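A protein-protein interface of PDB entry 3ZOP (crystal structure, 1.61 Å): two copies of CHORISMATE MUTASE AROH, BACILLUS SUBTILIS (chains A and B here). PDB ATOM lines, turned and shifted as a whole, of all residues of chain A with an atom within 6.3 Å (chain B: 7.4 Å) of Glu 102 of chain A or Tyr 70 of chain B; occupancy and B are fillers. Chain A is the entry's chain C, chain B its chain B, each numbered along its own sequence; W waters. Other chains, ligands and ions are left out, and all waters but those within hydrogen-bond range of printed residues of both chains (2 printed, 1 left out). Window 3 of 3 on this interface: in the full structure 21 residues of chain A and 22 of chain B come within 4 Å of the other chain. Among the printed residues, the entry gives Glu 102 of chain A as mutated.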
ATOM      1  N   GLY A   5     -17.445  -2.862 -17.314  1.00  0.00           N
ATOM      2  CA  GLY A   5     -18.898  -2.734 -17.237  1.00  0.00           C
ATOM      3  C   GLY A   5     -19.264  -1.542 -16.364  1.00  0.00           C
ATOM      4  O   GLY A   5     -18.622  -1.306 -15.332  1.00  0.00           O
ATOM      5  N   VAL A  99     -10.306   4.308 -17.174  1.00  0.00           N
ATOM      6  CA  VAL A  99     -10.687   4.580 -15.785  1.00  0.00           C
ATOM      7  C   VAL A  99     -10.597   3.301 -14.958  1.00  0.00           C
ATOM      8  O   VAL A  99     -11.120   2.261 -15.365  1.00  0.00           O
ATOM      9  CB  VAL A  99     -12.135   5.157 -15.682  1.00  0.00           C
ATOM     10  CG1 VAL A  99     -12.568   5.284 -14.231  1.00  0.00           C
ATOM     11  CG2 VAL A  99     -12.226   6.499 -16.370  1.00  0.00           C
ATOM     12  N   PRO A 100      -9.917   3.362 -13.798  1.00  0.00           N
ATOM     13  CA  PRO A 100      -9.783   2.162 -12.990  1.00  0.00           C
ATOM     14  C   PRO A 100     -11.122   1.686 -12.433  1.00  0.00           C
ATOM     15  O   PRO A 100     -12.057   2.472 -12.259  1.00  0.00           O
ATOM     16  CB  PRO A 100      -8.848   2.598 -11.855  1.00  0.00           C
ATOM     17  CG  PRO A 100      -9.011   4.077 -11.782  1.00  0.00           C
ATOM     18  CD  PRO A 100      -9.200   4.507 -13.209  1.00  0.00           C
ATOM     19  N   GLN A 101     -11.192   0.394 -12.159  1.00  0.00           N
ATOM     20  CA  GLN A 101     -12.410  -0.257 -11.726  1.00  0.00           C
ATOM     21  C   GLN A 101     -13.028   0.463 -10.528  1.00  0.00           C
ATOM     22  O   GLN A 101     -14.236   0.647 -10.468  1.00  0.00           O
ATOM     23  CB  GLN A 101     -12.094  -1.713 -11.386  1.00  0.00           C
ATOM     24  CG  GLN A 101     -13.280  -2.607 -11.103  1.00  0.00           C
ATOM     25  CD  GLN A 101     -12.840  -4.034 -10.789  1.00  0.00           C
ATOM     26  OE1 GLN A 101     -12.284  -4.303  -9.722  1.00  0.00           O
ATOM     27  NE2 GLN A 101     -13.084  -4.947 -11.718  1.00  0.00           N
ATOM     28  N   GLU A 102     -12.184   0.880  -9.585  1.00  0.00           N
ATOM     29  CA  GLU A 102     -12.640   1.562  -8.378  1.00  0.00           C
ATOM     30  C   GLU A 102     -13.279   2.914  -8.665  1.00  0.00           C
ATOM     31  O   GLU A 102     -14.029   3.433  -7.842  1.00  0.00           O
ATOM     32  CB  GLU A 102     -11.469   1.767  -7.402  1.00  0.00           C
ATOM     33  CG  GLU A 102     -10.777   0.489  -6.951  1.00  0.00           C
ATOM     34  CD  GLU A 102      -9.680   0.024  -7.901  1.00  0.00           C
ATOM     35  OE1 GLU A 102      -9.500   0.646  -8.971  1.00  0.00           O
ATOM     36  OE2 GLU A 102      -8.980  -0.966  -7.568  1.00  0.00           O
ATOM     37  N   GLN A 103     -12.972   3.497  -9.820  1.00  0.00           N
ATOM     38  CA  GLN A 103     -13.417   4.854 -10.108  1.00  0.00           C
ATOM     39  C   GLN A 103     -14.580   4.926 -11.080  1.00  0.00           C
ATOM     40  O   GLN A 103     -15.096   6.011 -11.345  1.00  0.00           O
ATOM     41  CB  GLN A 103     -12.254   5.722 -10.608  1.00  0.00           C
ATOM     42  CG  GLN A 103     -11.155   5.914  -9.573  1.00  0.00           C
ATOM     43  CD  GLN A 103     -10.194   7.030  -9.945  1.00  0.00           C
ATOM     44  OE1 GLN A 103     -10.057   7.395 -11.116  1.00  0.00           O
ATOM     45  NE2 GLN A 103      -9.522   7.579  -8.945  1.00  0.00           N
ATOM     46  N   ILE A 104     -14.993   3.778 -11.614  1.00  0.00           N
ATOM     47  CA  ILE A 104     -16.126   3.751 -12.524  1.00  0.00           C
ATOM     48  C   ILE A 104     -17.342   4.234 -11.753  1.00  0.00           C
ATOM     49  O   ILE A 104     -17.536   3.866 -10.590  1.00  0.00           O
ATOM     50  CB  ILE A 104     -16.381   2.338 -13.074  1.00  0.00           C
ATOM     51  CG1 ILE A 104     -15.184   1.883 -13.911  1.00  0.00           C
ATOM     52  CG2 ILE A 104     -17.658   2.309 -13.888  1.00  0.00           C
ATOM     53  CD1 ILE A 104     -15.020   2.625 -15.233  1.00  0.00           C
ATOM     54  N   HIS A 106     -20.976   3.970 -11.163  1.00  0.00           N
ATOM     55  CA  HIS A 106     -22.243   3.265 -11.331  1.00  0.00           C
ATOM     56  C   HIS A 106     -23.363   4.143 -10.784  1.00  0.00           C
ATOM     57  O   HIS A 106     -23.148   4.936  -9.853  1.00  0.00           O
ATOM     58  CB  HIS A 106     -22.194   1.908 -10.634  1.00  0.00           C
ATOM     59  CG  HIS A 106     -20.993   1.097 -11.014  1.00  0.00           C
ATOM     60  ND1 HIS A 106     -20.887   0.445 -12.226  1.00  0.00           N
ATOM     61  CD2 HIS A 106     -19.832   0.866 -10.358  1.00  0.00           C
ATOM     62  CE1 HIS A 106     -19.722  -0.175 -12.286  1.00  0.00           C
ATOM     63  NE2 HIS A 106     -19.061   0.068 -11.166  1.00  0.00           N
ATOM     64  N   PRO B  39      -9.504  -9.560  -9.447  1.00  0.00           N
ATOM     65  CA  PRO B  39     -10.733  -8.798  -9.681  1.00  0.00           C
ATOM     66  C   PRO B  39     -10.542  -7.609 -10.630  1.00  0.00           C
ATOM     67  O   PRO B  39     -11.427  -7.300 -11.435  1.00  0.00           O
ATOM     68  CB  PRO B  39     -11.139  -8.334  -8.268  1.00  0.00           C
ATOM     69  CG  PRO B  39      -9.869  -8.403  -7.455  1.00  0.00           C
ATOM     70  CD  PRO B  39      -9.137  -9.603  -8.017  1.00  0.00           C
ATOM     71  N   GLU B  40      -9.380  -6.965 -10.558  1.00  0.00           N
ATOM     72  CA  GLU B  40      -9.121  -5.800 -11.393  1.00  0.00           C
ATOM     73  C   GLU B  40      -9.145  -6.125 -12.896  1.00  0.00           C
ATOM     74  O   GLU B  40      -9.336  -5.236 -13.720  1.00  0.00           O
ATOM     75  CB  GLU B  40      -7.798  -5.141 -11.005  1.00  0.00           C
ATOM     76  CG  GLU B  40      -6.591  -6.043 -11.194  1.00  0.00           C
ATOM     77  CD  GLU B  40      -6.167  -6.776  -9.926  1.00  0.00           C
ATOM     78  OE1 GLU B  40      -7.009  -7.050  -9.022  1.00  0.00           O
ATOM     79  OE2 GLU B  40      -4.960  -7.068  -9.835  1.00  0.00           O
ATOM     80  N   VAL B  42     -11.316  -8.232 -14.235  1.00  0.00           N
ATOM     81  CA  VAL B  42     -12.683  -8.632 -14.598  1.00  0.00           C
ATOM     82  C   VAL B  42     -13.484  -7.456 -15.149  1.00  0.00           C
ATOM     83  O   VAL B  42     -13.731  -6.462 -14.463  1.00  0.00           O
ATOM     84  CB  VAL B  42     -13.408  -9.284 -13.414  1.00  0.00           C
ATOM     85  CG1 VAL B  42     -14.837  -9.665 -13.803  1.00  0.00           C
ATOM     86  CG2 VAL B  42     -12.622 -10.494 -12.933  1.00  0.00           C
ATOM     87  N   VAL B  43     -13.859  -7.561 -16.416  1.00  0.00           N
ATOM     88  CA  VAL B  43     -14.659  -6.537 -17.076  1.00  0.00           C
ATOM     89  C   VAL B  43     -16.029  -6.409 -16.389  1.00  0.00           C
ATOM     90  O   VAL B  43     -16.450  -5.315 -15.990  1.00  0.00           O
ATOM     91  CB  VAL B  43     -14.876  -6.930 -18.554  1.00  0.00           C
ATOM     92  CG1 VAL B  43     -15.776  -5.918 -19.253  1.00  0.00           C
ATOM     93  CG2 VAL B  43     -13.521  -7.059 -19.279  1.00  0.00           C
ATOM     94  N   VAL B  62     -20.949 -12.378  -4.476  1.00  0.00           N
ATOM     95  CA  VAL B  62     -19.745 -11.732  -5.003  1.00  0.00           C
ATOM     96  C   VAL B  62     -19.148 -10.795  -3.955  1.00  0.00           C
ATOM     97  O   VAL B  62     -17.928 -10.684  -3.839  1.00  0.00           O
ATOM     98  CB  VAL B  62     -20.022 -11.000  -6.334  1.00  0.00           C
ATOM     99  CG1 VAL B  62     -18.771 -10.274  -6.832  1.00  0.00           C
ATOM    100  CG2 VAL B  62     -20.497 -11.994  -7.365  1.00  0.00           C
ATOM    101  N   ARG B  63     -20.011 -10.152  -3.170  1.00  0.00           N
ATOM    102  CA  ARG B  63     -19.559  -9.279  -2.084  1.00  0.00           C
ATOM    103  C   ARG B  63     -18.920 -10.044  -0.921  1.00  0.00           C
ATOM    104  O   ARG B  63     -18.347  -9.441  -0.010  1.00  0.00           O
ATOM    105  CB  ARG B  63     -20.710  -8.398  -1.582  1.00  0.00           C
ATOM    106  CG  ARG B  63     -21.281  -7.486  -2.663  1.00  0.00           C
ATOM    107  CD  ARG B  63     -21.858  -6.204  -2.076  1.00  0.00           C
ATOM    108  NE  ARG B  63     -22.153  -5.215  -3.109  1.00  0.00           N
ATOM    109  CZ  ARG B  63     -23.379  -4.830  -3.456  1.00  0.00           C
ATOM    110  NH1 ARG B  63     -24.440  -5.345  -2.844  1.00  0.00           N
ATOM    111  NH2 ARG B  63     -23.546  -3.922  -4.410  1.00  0.00           N
ATOM    112  N   LEU B  65     -16.531 -12.126  -1.557  1.00  0.00           N
ATOM    113  CA  LEU B  65     -15.178 -12.315  -2.023  1.00  0.00           C
ATOM    114  C   LEU B  65     -14.440 -11.026  -1.755  1.00  0.00           C
ATOM    115  O   LEU B  65     -14.694 -10.008  -2.395  1.00  0.00           O
ATOM    116  CB  LEU B  65     -15.142 -12.622  -3.521  1.00  0.00           C
ATOM    117  CG  LEU B  65     -15.890 -13.839  -4.066  1.00  0.00           C
ATOM    118  CD1 LEU B  65     -16.127 -13.662  -5.555  1.00  0.00           C
ATOM    119  CD2 LEU B  65     -15.149 -15.131  -3.798  1.00  0.00           C
ATOM    120  N   GLY B  67     -12.114  -8.106  -2.012  1.00  0.00           N
ATOM    121  CA  GLY B  67     -11.440  -7.495  -3.143  1.00  0.00           C
ATOM    122  C   GLY B  67     -12.305  -7.388  -4.383  1.00  0.00           C
ATOM    123  O   GLY B  67     -11.944  -6.710  -5.341  1.00  0.00           O
ATOM    124  N   TRP B  68     -13.459  -8.043  -4.370  1.00  0.00           N
ATOM    125  CA  TRP B  68     -14.324  -8.062  -5.557  1.00  0.00           C
ATOM    126  C   TRP B  68     -15.465  -7.054  -5.521  1.00  0.00           C
ATOM    127  O   TRP B  68     -16.378  -7.133  -6.341  1.00  0.00           O
ATOM    128  CB  TRP B  68     -14.869  -9.476  -5.781  1.00  0.00           C
ATOM    129  CG  TRP B  68     -13.809 -10.392  -6.324  1.00  0.00           C
ATOM    130  CD1 TRP B  68     -12.637 -10.764  -5.711  1.00  0.00           C
ATOM    131  CD2 TRP B  68     -13.809 -11.027  -7.602  1.00  0.00           C
ATOM    132  NE1 TRP B  68     -11.916 -11.589  -6.536  1.00  0.00           N
ATOM    133  CE2 TRP B  68     -12.613 -11.770  -7.703  1.00  0.00           C
ATOM    134  CE3 TRP B  68     -14.705 -11.042  -8.675  1.00  0.00           C
ATOM    135  CZ2 TRP B  68     -12.293 -12.520  -8.835  1.00  0.00           C
ATOM    136  CZ3 TRP B  68     -14.385 -11.795  -9.797  1.00  0.00           C
ATOM    137  CH2 TRP B  68     -13.186 -12.517  -9.867  1.00  0.00           C
ATOM    138  N   GLN B  69     -15.399  -6.102  -4.588  1.00  0.00           N
ATOM    139  CA  GLN B  69     -16.512  -5.181  -4.349  1.00  0.00           C
ATOM    140  C   GLN B  69     -16.784  -4.188  -5.479  1.00  0.00           C
ATOM    141  O   GLN B  69     -17.848  -3.560  -5.508  1.00  0.00           O
ATOM    142  CB  GLN B  69     -16.315  -4.417  -3.040  1.00  0.00           C
ATOM    143  CG  GLN B  69     -15.079  -3.532  -3.019  1.00  0.00           C
ATOM    144  CD  GLN B  69     -13.872  -4.208  -2.373  1.00  0.00           C
ATOM    145  OE1 GLN B  69     -13.639  -5.408  -2.541  1.00  0.00           O
ATOM    146  NE2 GLN B  69     -13.103  -3.430  -1.618  1.00  0.00           N
ATOM    147  N   TYR B  70     -15.833  -4.040  -6.398  1.00  0.00           N
ATOM    148  CA  TYR B  70     -15.999  -3.128  -7.524  1.00  0.00           C
ATOM    149  C   TYR B  70     -16.245  -3.850  -8.838  1.00  0.00           C
ATOM    150  O   TYR B  70     -16.290  -3.221  -9.899  1.00  0.00           O
ATOM    151  CB  TYR B  70     -14.785  -2.222  -7.667  1.00  0.00           C
ATOM    152  CG  TYR B  70     -14.427  -1.474  -6.410  1.00  0.00           C
ATOM    153  CD1 TYR B  70     -15.190  -0.397  -5.976  1.00  0.00           C
ATOM    154  CD2 TYR B  70     -13.320  -1.841  -5.664  1.00  0.00           C
ATOM    155  CE1 TYR B  70     -14.855   0.295  -4.811  1.00  0.00           C
ATOM    156  CE2 TYR B  70     -12.978  -1.164  -4.505  1.00  0.00           C
ATOM    157  CZ  TYR B  70     -13.747  -0.100  -4.086  1.00  0.00           C
ATOM    158  OH  TYR B  70     -13.391   0.570  -2.943  1.00  0.00           O
ATOM    159  N   VAL B  71     -16.376  -5.171  -8.790  1.00  0.00           N
ATOM    160  CA  VAL B  71     -16.656  -5.919 -10.016  1.00  0.00           C
ATOM    161  C   VAL B  71     -18.140  -5.808 -10.343  1.00  0.00           C
ATOM    162  O   VAL B  71     -18.977  -6.189  -9.534  1.00  0.00           O
ATOM    163  CB  VAL B  71     -16.260  -7.413  -9.901  1.00  0.00           C
ATOM    164  CG1 VAL B  71     -16.682  -8.156 -11.166  1.00  0.00           C
ATOM    165  CG2 VAL B  71     -14.753  -7.549  -9.689  1.00  0.00           C
ATOM    166  N   PRO B  72     -18.480  -5.256 -11.526  1.00  0.00           N
ATOM    167  CA  PRO B  72     -19.905  -5.077 -11.824  1.00  0.00           C
ATOM    168  C   PRO B  72     -20.575  -6.384 -12.215  1.00  0.00           C
ATOM    169  O   PRO B  72     -20.024  -7.163 -12.995  1.00  0.00           O
ATOM    170  CB  PRO B  72     -19.908  -4.105 -13.008  1.00  0.00           C
ATOM    171  CG  PRO B  72     -18.596  -4.296 -13.667  1.00  0.00           C
ATOM    172  CD  PRO B  72     -17.613  -4.732 -12.599  1.00  0.00           C
ATOM    173  N   VAL B  73     -21.762  -6.622 -11.681  1.00  0.00           N
ATOM    174  CA  VAL B  73     -22.430  -7.877 -11.912  1.00  0.00           C
ATOM    175  C   VAL B  73     -23.915  -7.616 -12.085  1.00  0.00           C
ATOM    176  O   VAL B  73     -24.471  -6.698 -11.481  1.00  0.00           O
ATOM    177  CB  VAL B  73     -22.177  -8.827 -10.718  1.00  0.00           C
ATOM    178  CG1 VAL B  73     -22.450  -8.116  -9.408  1.00  0.00           C
ATOM    179  CG2 VAL B  73     -22.984 -10.125 -10.866  1.00  0.00           C
HETATM  180  O   HOH W   1     -14.310  -3.816 -14.190  1.00  0.00           O
HETATM  181  O   HOH W   2     -16.367  -0.915 -11.283  1.00  0.00           O
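Of the 14 printed residues of chain B, 7 touch a printed residue of chain A.
Printed residues of chain B that touch a printed residue of chain A: Pro 39, Glu 40, Val 42, Val 43, Tyr 70, Val 71 and Pro 72.
Pro 72 of chain B touches Gly 5 of chain A (CG to O, 3.4 Å).
Gln 101 of chain A touches Glu 40 of chain B.
O of Tyr 70 of chain B touches CG of Gln 101 of chain A, at 3.3 Å.
Gln 101 of chain A touches Val 71 of chain B (NE2 to CG2, 3.7 Å).
Glu 102 of chain A touches Tyr 70 of chain B.
O of Val 42 of chain B is in hydrogen-bond range of NE2 of Gln 101 of chain A, at 3.2 Å.
The backbone carbonyl oxygen (O) of Val 43 of chain B is in hydrogen-bond range of the backbone NH (N) of Gly 5 of chain A (3.0 Å).
The side-chain amide nitrogen (NE2) of Gln 101 of chain A is in hydrogen-bond range of the backbone carbonyl oxygen (O) of Pro 39 of chain B (2.9 Å).
No position is printed for both chains.
Of the 8 pairs that touch across the chains among the printed residues, none has its exchanged pair printed and touching as well.
Water W2 lies within hydrogen-bond range of O of Tyr 70 of chain B, O of Gln 101 of chain A and NE2 of His 106 of chain A.
Water W1 lies within hydrogen-bond range of O of Val 42 of chain B (2.7 Å), NE2 of Gln 101 of chain A (3.0 Å) and O of Val 43 of chain B (3.2 Å).
Of the printed residues of chain B, Gly 5 of chain A touches Val 43 and Pro 72.
Val 99 of chain A touches none of the printed residues of chain B.
Glu 102 of chain A touches one residue of chain B.
Printed residues of chain A within 4 Å of Pro 39 of chain B: Gln 101 (2.9 Å).
Printed residues of chain A within 4 Å of Val 42 of chain B: Gln 101.
Of chain A, only Gln 101 and Glu 102 come within 4 Å of Tyr 70 of chain B.
Printed residues of chain A within 4 Å of Pro 72 of chain B: Gly 5.
The nearest printed residue of chain A that does not touch Pro 39 of chain B is Glu 102 of chain A (7.5 Å).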
